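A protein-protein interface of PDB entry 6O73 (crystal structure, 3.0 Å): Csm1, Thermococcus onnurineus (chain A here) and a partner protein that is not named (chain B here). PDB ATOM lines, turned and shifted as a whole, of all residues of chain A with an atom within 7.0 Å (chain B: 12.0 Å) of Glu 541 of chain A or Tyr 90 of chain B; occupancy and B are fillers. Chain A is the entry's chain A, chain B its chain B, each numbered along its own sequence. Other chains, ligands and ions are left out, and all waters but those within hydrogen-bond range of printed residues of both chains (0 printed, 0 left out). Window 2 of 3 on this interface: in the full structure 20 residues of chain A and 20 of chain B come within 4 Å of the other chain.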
ATOM      1  N   LYS A 371      -3.474   6.884   4.965  1.00  0.00           N
ATOM      2  CA  LYS A 371      -2.775   5.612   5.297  1.00  0.00           C
ATOM      3  C   LYS A 371      -2.638   4.727   4.050  1.00  0.00           C
ATOM      4  O   LYS A 371      -1.639   3.985   3.976  1.00  0.00           O
ATOM      5  CB  LYS A 371      -3.525   4.870   6.406  1.00  0.00           C
ATOM      6  CG  LYS A 371      -2.797   3.662   6.970  1.00  0.00           C
ATOM      7  CD  LYS A 371      -3.271   3.274   8.350  1.00  0.00           C
ATOM      8  CE  LYS A 371      -2.234   2.487   9.122  1.00  0.00           C
ATOM      9  NZ  LYS A 371      -2.717   2.135  10.477  1.00  0.00           N
ATOM     10  N   ASP A 537       9.429  13.392  17.740  1.00  0.00           N
ATOM     11  CA  ASP A 537       9.112  12.006  18.165  1.00  0.00           C
ATOM     12  C   ASP A 537       7.684  11.651  17.753  1.00  0.00           C
ATOM     13  O   ASP A 537       6.767  12.432  18.057  1.00  0.00           O
ATOM     14  CB  ASP A 537       9.295  11.832  19.673  1.00  0.00           C
ATOM     15  CG  ASP A 537      10.748  11.780  20.116  1.00  0.00           C
ATOM     16  OD1 ASP A 537      11.596  11.321  19.312  1.00  0.00           O
ATOM     17  OD2 ASP A 537      11.019  12.185  21.264  1.00  0.00           O
ATOM     18  N   ARG A 538       7.521  10.499  17.099  1.00  0.00           N
ATOM     19  CA  ARG A 538       6.205   9.917  16.734  1.00  0.00           C
ATOM     20  C   ARG A 538       5.364  10.991  16.037  1.00  0.00           C
ATOM     21  O   ARG A 538       4.160  11.094  16.330  1.00  0.00           O
ATOM     22  CB  ARG A 538       5.539   9.357  17.993  1.00  0.00           C
ATOM     23  CG  ARG A 538       6.256   8.138  18.555  1.00  0.00           C
ATOM     24  CD  ARG A 538       5.691   7.626  19.864  1.00  0.00           C
ATOM     25  NE  ARG A 538       6.342   6.385  20.274  1.00  0.00           N
ATOM     26  CZ  ARG A 538       6.345   5.886  21.511  1.00  0.00           C
ATOM     27  NH1 ARG A 538       6.973   4.750  21.765  1.00  0.00           N
ATOM     28  NH2 ARG A 538       5.731   6.520  22.496  1.00  0.00           N
ATOM     29  N   LEU A 539       5.989  11.772  15.155  1.00  0.00           N
ATOM     30  CA  LEU A 539       5.334  12.901  14.450  1.00  0.00           C
ATOM     31  C   LEU A 539       4.335  12.368  13.417  1.00  0.00           C
ATOM     32  O   LEU A 539       3.321  13.050  13.181  1.00  0.00           O
ATOM     33  CB  LEU A 539       6.399  13.765  13.777  1.00  0.00           C
ATOM     34  CG  LEU A 539       5.849  14.971  13.021  1.00  0.00           C
ATOM     35  CD1 LEU A 539       5.359  16.038  13.981  1.00  0.00           C
ATOM     36  CD2 LEU A 539       6.895  15.542  12.089  1.00  0.00           C
ATOM     37  N   GLY A 540       4.624  11.217  12.802  1.00  0.00           N
ATOM     38  CA  GLY A 540       3.705  10.529  11.875  1.00  0.00           C
ATOM     39  C   GLY A 540       2.426  10.104  12.577  1.00  0.00           C
ATOM     40  O   GLY A 540       1.364  10.123  11.926  1.00  0.00           O
ATOM     41  N   GLU A 541       2.524   9.739  13.859  1.00  0.00           N
ATOM     42  CA  GLU A 541       1.366   9.373  14.717  1.00  0.00           C
ATOM     43  C   GLU A 541       0.474  10.602  14.914  1.00  0.00           C
ATOM     44  O   GLU A 541      -0.749  10.488  14.698  1.00  0.00           O
ATOM     45  CB  GLU A 541       1.846   8.841  16.068  1.00  0.00           C
ATOM     46  CG  GLU A 541       0.728   8.681  17.081  1.00  0.00           C
ATOM     47  CD  GLU A 541       1.081   7.806  18.269  1.00  0.00           C
ATOM     48  OE1 GLU A 541       2.271   7.446  18.403  1.00  0.00           O
ATOM     49  OE2 GLU A 541       0.162   7.481  19.049  1.00  0.00           O
ATOM     50  N   PHE A 542       1.079  11.712  15.342  1.00  0.00           N
ATOM     51  CA  PHE A 542       0.435  13.028  15.588  1.00  0.00           C
ATOM     52  C   PHE A 542      -0.349  13.464  14.346  1.00  0.00           C
ATOM     53  O   PHE A 542      -1.574  13.659  14.450  1.00  0.00           O
ATOM     54  CB  PHE A 542       1.510  14.051  15.956  1.00  0.00           C
ATOM     55  CG  PHE A 542       1.029  15.462  16.171  1.00  0.00           C
ATOM     56  CD1 PHE A 542       0.143  15.763  17.193  1.00  0.00           C
ATOM     57  CD2 PHE A 542       1.504  16.499  15.381  1.00  0.00           C
ATOM     58  CE1 PHE A 542      -0.274  17.068  17.405  1.00  0.00           C
ATOM     59  CE2 PHE A 542       1.087  17.803  15.595  1.00  0.00           C
ATOM     60  CZ  PHE A 542       0.198  18.085  16.605  1.00  0.00           C
ATOM     61  N   PHE A 543       0.334  13.595  13.206  1.00  0.00           N
ATOM     62  CA  PHE A 543      -0.271  14.012  11.913  1.00  0.00           C
ATOM     63  C   PHE A 543      -1.421  13.067  11.547  1.00  0.00           C
ATOM     64  O   PHE A 543      -2.433  13.551  11.007  1.00  0.00           O
ATOM     65  CB  PHE A 543       0.784  14.096  10.803  1.00  0.00           C
ATOM     66  CG  PHE A 543       1.639  15.337  10.861  1.00  0.00           C
ATOM     67  CD1 PHE A 543       1.105  16.543  11.290  1.00  0.00           C
ATOM     68  CD2 PHE A 543       2.973  15.310  10.483  1.00  0.00           C
ATOM     69  CE1 PHE A 543       1.885  17.685  11.350  1.00  0.00           C
ATOM     70  CE2 PHE A 543       3.750  16.458  10.539  1.00  0.00           C
ATOM     71  CZ  PHE A 543       3.205  17.643  10.974  1.00  0.00           C
ATOM     72  N   SER A 544      -1.283  11.774  11.847  1.00  0.00           N
ATOM     73  CA  SER A 544      -2.313  10.739  11.570  1.00  0.00           C
ATOM     74  C   SER A 544      -3.488  10.849  12.556  1.00  0.00           C
ATOM     75  O   SER A 544      -4.486  10.136  12.335  1.00  0.00           O
ATOM     76  CB  SER A 544      -1.711   9.358  11.586  1.00  0.00           C
ATOM     77  OG  SER A 544      -2.667   8.386  11.195  1.00  0.00           O
ATOM     78  N   SER A 545      -3.392  11.693  13.595  1.00  0.00           N
ATOM     79  CA  SER A 545      -4.446  11.865  14.636  1.00  0.00           C
ATOM     80  C   SER A 545      -5.446  12.951  14.223  1.00  0.00           C
ATOM     81  O   SER A 545      -6.515  13.030  14.865  1.00  0.00           O
ATOM     82  CB  SER A 545      -3.860  12.172  15.997  1.00  0.00           C
ATOM     83  OG  SER A 545      -3.507  13.544  16.113  1.00  0.00           O
ATOM     84  N   MET A 546      -5.118  13.761  13.212  1.00  0.00           N
ATOM     85  CA  MET A 546      -5.956  14.914  12.790  1.00  0.00           C
ATOM     86  C   MET A 546      -7.186  14.380  12.041  1.00  0.00           C
ATOM     87  O   MET A 546      -7.018  13.510  11.159  1.00  0.00           O
ATOM     88  CB  MET A 546      -5.168  15.891  11.912  1.00  0.00           C
ATOM     89  CG  MET A 546      -3.823  16.306  12.500  1.00  0.00           C
ATOM     90  SD  MET A 546      -3.859  16.747  14.262  1.00  0.00           S
ATOM     91  CE  MET A 546      -4.630  18.361  14.188  1.00  0.00           C
ATOM     92  N   ARG A 666      11.800   7.000  23.799  1.00  0.00           N
ATOM     93  CA  ARG A 666      12.046   8.297  23.115  1.00  0.00           C
ATOM     94  C   ARG A 666      12.172   9.405  24.159  1.00  0.00           C
ATOM     95  O   ARG A 666      12.287   9.081  25.357  1.00  0.00           O
ATOM     96  CB  ARG A 666      10.942   8.581  22.097  1.00  0.00           C
ATOM     97  CG  ARG A 666      11.216   7.979  20.730  1.00  0.00           C
ATOM     98  CD  ARG A 666       9.935   7.746  19.956  1.00  0.00           C
ATOM     99  NE  ARG A 666      10.227   7.308  18.598  1.00  0.00           N
ATOM    100  CZ  ARG A 666      10.431   6.044  18.222  1.00  0.00           C
ATOM    101  NH1 ARG A 666      10.705   5.773  16.957  1.00  0.00           N
ATOM    102  NH2 ARG A 666      10.355   5.055  19.099  1.00  0.00           N
ATOM    103  N   LYS B  69      17.122  -9.537   5.004  1.00  0.00           N
ATOM    104  CA  LYS B  69      15.657  -9.334   5.118  1.00  0.00           C
ATOM    105  C   LYS B  69      15.092  -9.124   3.718  1.00  0.00           C
ATOM    106  O   LYS B  69      15.479  -8.186   3.028  1.00  0.00           O
ATOM    107  CB  LYS B  69      15.383  -8.134   6.026  1.00  0.00           C
ATOM    108  CG  LYS B  69      14.069  -7.415   5.786  1.00  0.00           C
ATOM    109  CD  LYS B  69      14.213  -5.927   5.941  1.00  0.00           C
ATOM    110  CE  LYS B  69      12.883  -5.215   5.973  1.00  0.00           C
ATOM    111  NZ  LYS B  69      12.084  -5.628   7.153  1.00  0.00           N
ATOM    112  N   VAL B  73       8.619  -7.869   2.795  1.00  0.00           N
ATOM    113  CA  VAL B  73       7.956  -7.717   4.127  1.00  0.00           C
ATOM    114  C   VAL B  73       7.609  -6.245   4.365  1.00  0.00           C
ATOM    115  O   VAL B  73       6.691  -5.990   5.175  1.00  0.00           O
ATOM    116  CB  VAL B  73       8.816  -8.259   5.283  1.00  0.00           C
ATOM    117  CG1 VAL B  73       9.283  -9.682   5.025  1.00  0.00           C
ATOM    118  CG2 VAL B  73       9.996  -7.353   5.599  1.00  0.00           C
ATOM    119  N   GLU B  74       8.324  -5.326   3.709  1.00  0.00           N
ATOM    120  CA  GLU B  74       8.220  -3.862   3.952  1.00  0.00           C
ATOM    121  C   GLU B  74       6.785  -3.383   3.716  1.00  0.00           C
ATOM    122  O   GLU B  74       6.205  -2.772   4.608  1.00  0.00           O
ATOM    123  CB  GLU B  74       9.268  -3.114   3.125  1.00  0.00           C
ATOM    124  CG  GLU B  74      10.688  -3.355   3.612  1.00  0.00           C
ATOM    125  CD  GLU B  74      11.545  -2.110   3.732  1.00  0.00           C
ATOM    126  OE1 GLU B  74      11.012  -1.074   4.155  1.00  0.00           O
ATOM    127  OE2 GLU B  74      12.740  -2.182   3.396  1.00  0.00           O
ATOM    128  N   LEU B  77       3.738  -4.929   6.417  1.00  0.00           N
ATOM    129  CA  LEU B  77       4.123  -4.916   7.857  1.00  0.00           C
ATOM    130  C   LEU B  77       2.880  -4.975   8.752  1.00  0.00           C
ATOM    131  O   LEU B  77       2.919  -5.709   9.760  1.00  0.00           O
ATOM    132  CB  LEU B  77       4.984  -3.684   8.151  1.00  0.00           C
ATOM    133  CG  LEU B  77       6.425  -3.817   7.666  1.00  0.00           C
ATOM    134  CD1 LEU B  77       7.105  -2.465   7.546  1.00  0.00           C
ATOM    135  CD2 LEU B  77       7.211  -4.739   8.583  1.00  0.00           C
ATOM    136  N   GLU B  78       1.810  -4.270   8.383  1.00  0.00           N
ATOM    137  CA  GLU B  78       0.594  -4.132   9.227  1.00  0.00           C
ATOM    138  C   GLU B  78      -0.199  -5.448   9.202  1.00  0.00           C
ATOM    139  O   GLU B  78      -0.896  -5.726  10.199  1.00  0.00           O
ATOM    140  CB  GLU B  78      -0.181  -2.890   8.786  1.00  0.00           C
ATOM    141  CG  GLU B  78       0.652  -1.623   8.914  1.00  0.00           C
ATOM    142  CD  GLU B  78       0.028  -0.367   8.338  1.00  0.00           C
ATOM    143  OE1 GLU B  78      -1.128  -0.435   7.878  1.00  0.00           O
ATOM    144  OE2 GLU B  78       0.707   0.675   8.342  1.00  0.00           O
ATOM    145  N   GLY B  79      -0.062  -6.245   8.135  1.00  0.00           N
ATOM    146  CA  GLY B  79      -0.556  -7.635   8.064  1.00  0.00           C
ATOM    147  C   GLY B  79       0.009  -8.501   9.182  1.00  0.00           C
ATOM    148  O   GLY B  79       1.211  -8.830   9.112  1.00  0.00           O
ATOM    149  N   ASP B  85      -1.798  -2.546  18.977  1.00  0.00           N
ATOM    150  CA  ASP B  85      -1.516  -1.247  19.649  1.00  0.00           C
ATOM    151  C   ASP B  85      -1.130  -0.203  18.590  1.00  0.00           C
ATOM    152  O   ASP B  85      -0.583  -0.604  17.545  1.00  0.00           O
ATOM    153  CB  ASP B  85      -0.421  -1.415  20.708  1.00  0.00           C
ATOM    154  CG  ASP B  85      -0.042  -0.144  21.455  1.00  0.00           C
ATOM    155  OD1 ASP B  85      -0.813   0.833  21.390  1.00  0.00           O
ATOM    156  OD2 ASP B  85       1.021  -0.145  22.102  1.00  0.00           O
ATOM    157  N   GLU B  86      -1.413   1.079  18.854  1.00  0.00           N
ATOM    158  CA  GLU B  86      -0.969   2.234  18.021  1.00  0.00           C
ATOM    159  C   GLU B  86       0.546   2.419  18.188  1.00  0.00           C
ATOM    160  O   GLU B  86       1.278   2.167  17.211  1.00  0.00           O
ATOM    161  CB  GLU B  86      -1.692   3.533  18.402  1.00  0.00           C
ATOM    162  CG  GLU B  86      -2.980   3.788  17.635  1.00  0.00           C
ATOM    163  CD  GLU B  86      -3.630   5.139  17.906  1.00  0.00           C
ATOM    164  OE1 GLU B  86      -4.022   5.819  16.933  1.00  0.00           O
ATOM    165  OE2 GLU B  86      -3.751   5.511  19.093  1.00  0.00           O
ATOM    166  N   GLU B  87       0.989   2.824  19.388  1.00  0.00           N
ATOM    167  CA  GLU B  87       2.389   3.253  19.673  1.00  0.00           C
ATOM    168  C   GLU B  87       3.315   2.042  19.856  1.00  0.00           C
ATOM    169  O   GLU B  87       4.488   2.268  20.224  1.00  0.00           O
ATOM    170  CB  GLU B  87       2.450   4.161  20.904  1.00  0.00           C
ATOM    171  CG  GLU B  87       1.667   5.446  20.738  1.00  0.00           C
ATOM    172  CD  GLU B  87       2.050   6.569  21.688  1.00  0.00           C
ATOM    173  OE1 GLU B  87       1.260   6.864  22.604  1.00  0.00           O
ATOM    174  OE2 GLU B  87       3.130   7.157  21.500  1.00  0.00           O
ATOM    175  N   GLU B  88       2.832   0.818  19.615  1.00  0.00           N
ATOM    176  CA  GLU B  88       3.700  -0.381  19.450  1.00  0.00           C
ATOM    177  C   GLU B  88       3.876  -0.688  17.958  1.00  0.00           C
ATOM    178  O   GLU B  88       4.956  -1.202  17.598  1.00  0.00           O
ATOM    179  CB  GLU B  88       3.146  -1.601  20.186  1.00  0.00           C
ATOM    180  CG  GLU B  88       3.571  -1.676  21.641  1.00  0.00           C
ATOM    181  CD  GLU B  88       5.067  -1.828  21.864  1.00  0.00           C
ATOM    182  OE1 GLU B  88       5.765  -2.292  20.937  1.00  0.00           O
ATOM    183  OE2 GLU B  88       5.534  -1.473  22.965  1.00  0.00           O
ATOM    184  N   ARG B  89       2.867  -0.397  17.128  1.00  0.00           N
ATOM    185  CA  ARG B  89       2.933  -0.627  15.658  1.00  0.00           C
ATOM    186  C   ARG B  89       3.927   0.357  15.031  1.00  0.00           C
ATOM    187  O   ARG B  89       4.712  -0.097  14.184  1.00  0.00           O
ATOM    188  CB  ARG B  89       1.552  -0.536  15.000  1.00  0.00           C
ATOM    189  CG  ARG B  89       0.837  -1.876  14.898  1.00  0.00           C
ATOM    190  CD  ARG B  89      -0.566  -1.745  14.340  1.00  0.00           C
ATOM    191  NE  ARG B  89      -1.387  -2.925  14.584  1.00  0.00           N
ATOM    192  CZ  ARG B  89      -2.711  -2.976  14.445  1.00  0.00           C
ATOM    193  NH1 ARG B  89      -3.388  -1.905  14.064  1.00  0.00           N
ATOM    194  NH2 ARG B  89      -3.357  -4.103  14.692  1.00  0.00           N
ATOM    195  N   TYR B  90       3.913   1.636  15.429  1.00  0.00           N
ATOM    196  CA  TYR B  90       4.827   2.679  14.887  1.00  0.00           C
ATOM    197  C   TYR B  90       6.281   2.227  15.057  1.00  0.00           C
ATOM    198  O   TYR B  90       6.965   2.028  14.030  1.00  0.00           O
ATOM    199  CB  TYR B  90       4.618   4.041  15.557  1.00  0.00           C
ATOM    200  CG  TYR B  90       3.323   4.720  15.198  1.00  0.00           C
ATOM    201  CD1 TYR B  90       3.067   5.138  13.901  1.00  0.00           C
ATOM    202  CD2 TYR B  90       2.347   4.944  16.156  1.00  0.00           C
ATOM    203  CE1 TYR B  90       1.872   5.754  13.565  1.00  0.00           C
ATOM    204  CE2 TYR B  90       1.147   5.556  15.837  1.00  0.00           C
ATOM    205  CZ  TYR B  90       0.907   5.963  14.536  1.00  0.00           C
ATOM    206  OH  TYR B  90      -0.271   6.571  14.213  1.00  0.00           O
ATOM    207  N   THR B  91       6.724   2.048  16.307  1.00  0.00           N
ATOM    208  CA  THR B  91       8.160   1.920  16.679  1.00  0.00           C
ATOM    209  C   THR B  91       8.750   0.670  16.019  1.00  0.00           C
ATOM    210  O   THR B  91       9.702   0.824  15.225  1.00  0.00           O
ATOM    211  CB  THR B  91       8.364   1.920  18.200  1.00  0.00           C
ATOM    212  OG1 THR B  91       7.788   0.742  18.761  1.00  0.00           O
ATOM    213  CG2 THR B  91       7.772   3.147  18.857  1.00  0.00           C
ATOM    214  N   THR B  92       8.190  -0.505  16.313  1.00  0.00           N
ATOM    215  CA  THR B  92       8.689  -1.816  15.816  1.00  0.00           C
ATOM    216  C   THR B  92       8.677  -1.807  14.281  1.00  0.00           C
ATOM    217  O   THR B  92       9.725  -2.148  13.704  1.00  0.00           O
ATOM    218  CB  THR B  92       7.913  -2.989  16.431  1.00  0.00           C
ATOM    219  OG1 THR B  92       6.524  -2.801  16.166  1.00  0.00           O
ATOM    220  CG2 THR B  92       8.123  -3.115  17.925  1.00  0.00           C
ATOM    221  N   ALA B  93       7.573  -1.386  13.649  1.00  0.00           N
ATOM    222  CA  ALA B  93       7.399  -1.380  12.173  1.00  0.00           C
ATOM    223  C   ALA B  93       8.465  -0.510  11.498  1.00  0.00           C
ATOM    224  O   ALA B  93       8.783  -0.804  10.331  1.00  0.00           O
ATOM    225  CB  ALA B  93       6.016  -0.927  11.774  1.00  0.00           C
ATOM    226  N   LYS B  94       8.986   0.518  12.175  1.00  0.00           N
ATOM    227  CA  LYS B  94      10.139   1.304  11.659  1.00  0.00           C
ATOM    228  C   LYS B  94      11.419   0.483  11.840  1.00  0.00           C
ATOM    229  O   LYS B  94      12.246   0.496  10.907  1.00  0.00           O
ATOM    230  CB  LYS B  94      10.251   2.684  12.314  1.00  0.00           C
ATOM    231  CG  LYS B  94       9.484   3.786  11.595  1.00  0.00           C
ATOM    232  CD  LYS B  94       9.962   5.185  11.916  1.00  0.00           C
ATOM    233  CE  LYS B  94       9.290   6.240  11.064  1.00  0.00           C
ATOM    234  NZ  LYS B  94       7.814   6.171  11.175  1.00  0.00           N
ATOM    235  N   ARG B  95      11.573  -0.217  12.971  1.00  0.00           N
ATOM    236  CA  ARG B  95      12.797  -1.014  13.264  1.00  0.00           C
ATOM    237  C   ARG B  95      12.820  -2.263  12.370  1.00  0.00           C
ATOM    238  O   ARG B  95      13.926  -2.793  12.155  1.00  0.00           O
ATOM    239  CB  ARG B  95      12.925  -1.398  14.744  1.00  0.00           C
ATOM    240  CG  ARG B  95      12.634  -0.299  15.761  1.00  0.00           C
ATOM    241  CD  ARG B  95      13.057   1.130  15.439  1.00  0.00           C
ATOM    242  NE  ARG B  95      14.498   1.371  15.462  1.00  0.00           N
ATOM    243  CZ  ARG B  95      15.078   2.568  15.595  1.00  0.00           C
ATOM    244  NH1 ARG B  95      14.353   3.665  15.749  1.00  0.00           N
ATOM    245  NH2 ARG B  95      16.396   2.656  15.598  1.00  0.00           N
ATOM    246  N   LEU B  96      11.665  -2.721  11.862  1.00  0.00           N
ATOM    247  CA  LEU B  96      11.590  -3.807  10.840  1.00  0.00           C
ATOM    248  C   LEU B  96      11.972  -3.220   9.476  1.00  0.00           C
ATOM    249  O   LEU B  96      12.711  -3.898   8.747  1.00  0.00           O
ATOM    250  CB  LEU B  96      10.193  -4.439  10.786  1.00  0.00           C
ATOM    251  CG  LEU B  96       9.662  -5.060  12.081  1.00  0.00           C
ATOM    252  CD1 LEU B  96       8.147  -5.178  12.042  1.00  0.00           C
ATOM    253  CD2 LEU B  96      10.274  -6.423  12.346  1.00  0.00           C
ATOM    254  N   ARG B  97      11.499  -2.010   9.152  1.00  0.00           N
ATOM    255  CA  ARG B  97      11.838  -1.284   7.894  1.00  0.00           C
ATOM    256  C   ARG B  97      13.337  -0.952   7.874  1.00  0.00           C
ATOM    257  O   ARG B  97      13.921  -0.952   6.772  1.00  0.00           O
ATOM    258  CB  ARG B  97      11.001  -0.008   7.740  1.00  0.00           C
ATOM    259  CG  ARG B  97      11.390   0.868   6.554  1.00  0.00           C
ATOM    260  CD  ARG B  97      10.485   2.073   6.371  1.00  0.00           C
ATOM    261  NE  ARG B  97       9.076   1.716   6.490  1.00  0.00           N
ATOM    262  CZ  ARG B  97       8.346   1.124   5.545  1.00  0.00           C
ATOM    263  NH1 ARG B  97       7.074   0.842   5.779  1.00  0.00           N
ATOM    264  NH2 ARG B  97       8.877   0.814   4.374  1.00  0.00           N
ATOM    265  N   LYS B  98      13.933  -0.670   9.038  1.00  0.00           N
ATOM    266  CA  LYS B  98      15.385  -0.365   9.168  1.00  0.00           C
ATOM    267  C   LYS B  98      16.197  -1.661   9.070  1.00  0.00           C
ATOM    268  O   LYS B  98      17.254  -1.631   8.413  1.00  0.00           O
ATOM    269  CB  LYS B  98      15.687   0.387  10.469  1.00  0.00           C
ATOM    270  CG  LYS B  98      15.474   1.892  10.381  1.00  0.00           C
ATOM    271  CD  LYS B  98      15.474   2.613  11.712  1.00  0.00           C
ATOM    272  CE  LYS B  98      14.941   4.026  11.592  1.00  0.00           C
ATOM    273  NZ  LYS B  98      14.865   4.705  12.906  1.00  0.00           N
ATOM    274  N   ALA B  99      15.726  -2.752   9.687  1.00  0.00           N
ATOM    275  CA  ALA B  99      16.457  -4.039   9.776  1.00  0.00           C
ATOM    276  C   ALA B  99      17.038  -4.393   8.405  1.00  0.00           C
ATOM    277  O   ALA B  99      16.290  -4.321   7.414  1.00  0.00           O
ATOM    278  CB  ALA B  99      15.556  -5.136  10.282  1.00  0.00           C
ATOM    279  N   ILE B 118      13.577  -9.445  15.056  1.00  0.00           N
ATOM    280  CA  ILE B 118      14.847  -8.866  14.528  1.00  0.00           C
ATOM    281  C   ILE B 118      16.000  -9.342  15.404  1.00  0.00           C
ATOM    282  O   ILE B 118      15.817  -9.567  16.599  1.00  0.00           O
ATOM    283  CB  ILE B 118      14.734  -7.328  14.485  1.00  0.00           C
ATOM    284  CG1 ILE B 118      13.517  -6.892  13.669  1.00  0.00           C
ATOM    285  CG2 ILE B 118      16.003  -6.680  13.956  1.00  0.00           C
ATOM    286  CD1 ILE B 118      13.501  -7.474  12.269  1.00  0.00           C
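N of Glu 87 of chain B sits at hydrogen-bond distance from OD1 of Asp 85 of chain B (3.3 Å).
Arg 538 of chain A touches Thr 91 of chain B. OH of Tyr 90 of chain B touches CA of Glu 541 of chain A, 3.3 Å away. Thr 91 of chain B touches Arg 666 of chain A.
Of chain A, only Glu 541 comes within 4 Å of Tyr 90 of chain B. Of chain B, only Glu 87 and Thr 91 come within 4 Å of Arg 538 of chain A. No residue of chain B comes within 4 Å of Leu 539 of chain A. No residue of chain B comes within 4 Å of Gly 540 of chain A. No residue of chain B comes within 4 Å of Phe 542 of chain A. Of the printed residues of chain A, Glu 78 of chain B touches Lys 371 (3.4 Å). Of the printed residues of chain A, Glu 87 of chain B touches Arg 538 and Glu 541. Printed residues of chain A within 4 Å of Thr 91 of chain B: Arg 538 (3.4 Å) and Arg 666 (3.2 Å). Of the printed residues of chain B, Lys 371 of chain A touches Glu 78 (3.4 Å). Of the printed residues of chain B, Arg 666 of chain A touches Thr 91 (3.2 Å). Asp 85 of chain B touches none of the printed residues of chain A. Leu 77 of chain B touches none of the printed residues of chain A. The nearest residue of chain B that does not touch Glu 541 of chain A is Glu 86 of chain B (4.4 Å).
OE1 of Glu 541 of chain A sits close to OE2 of Glu 87 of chain B. The side-chain amino group of Lys 371 of chain A is in salt-bridge range of the side-chain carboxylate of Glu 78 of chain B. The side-chain carboxylate of Glu 87 of chain B lies within salt-bridge range of the guanidinium group of Arg 538 of chain A (2.9 Å).
Of the 22 printed residues of chain B, 4 touch a printed residue of chain A. Printed residues of chain A that touch a printed residue of chain B: Lys 371, Arg 538, Glu 541 and Arg 666. Among the printed residues, 6 pairs touch across the chains. Among the printed residues, Asp or Glu carboxylates within 4 Å of a Lys or Arg side-chain nitrogen of the other chain: Lys 371 of chain A with Glu 78 of chain B (3.99 Å) and Arg 538 of chain A with Glu 87 of chain B (2.9 Å).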
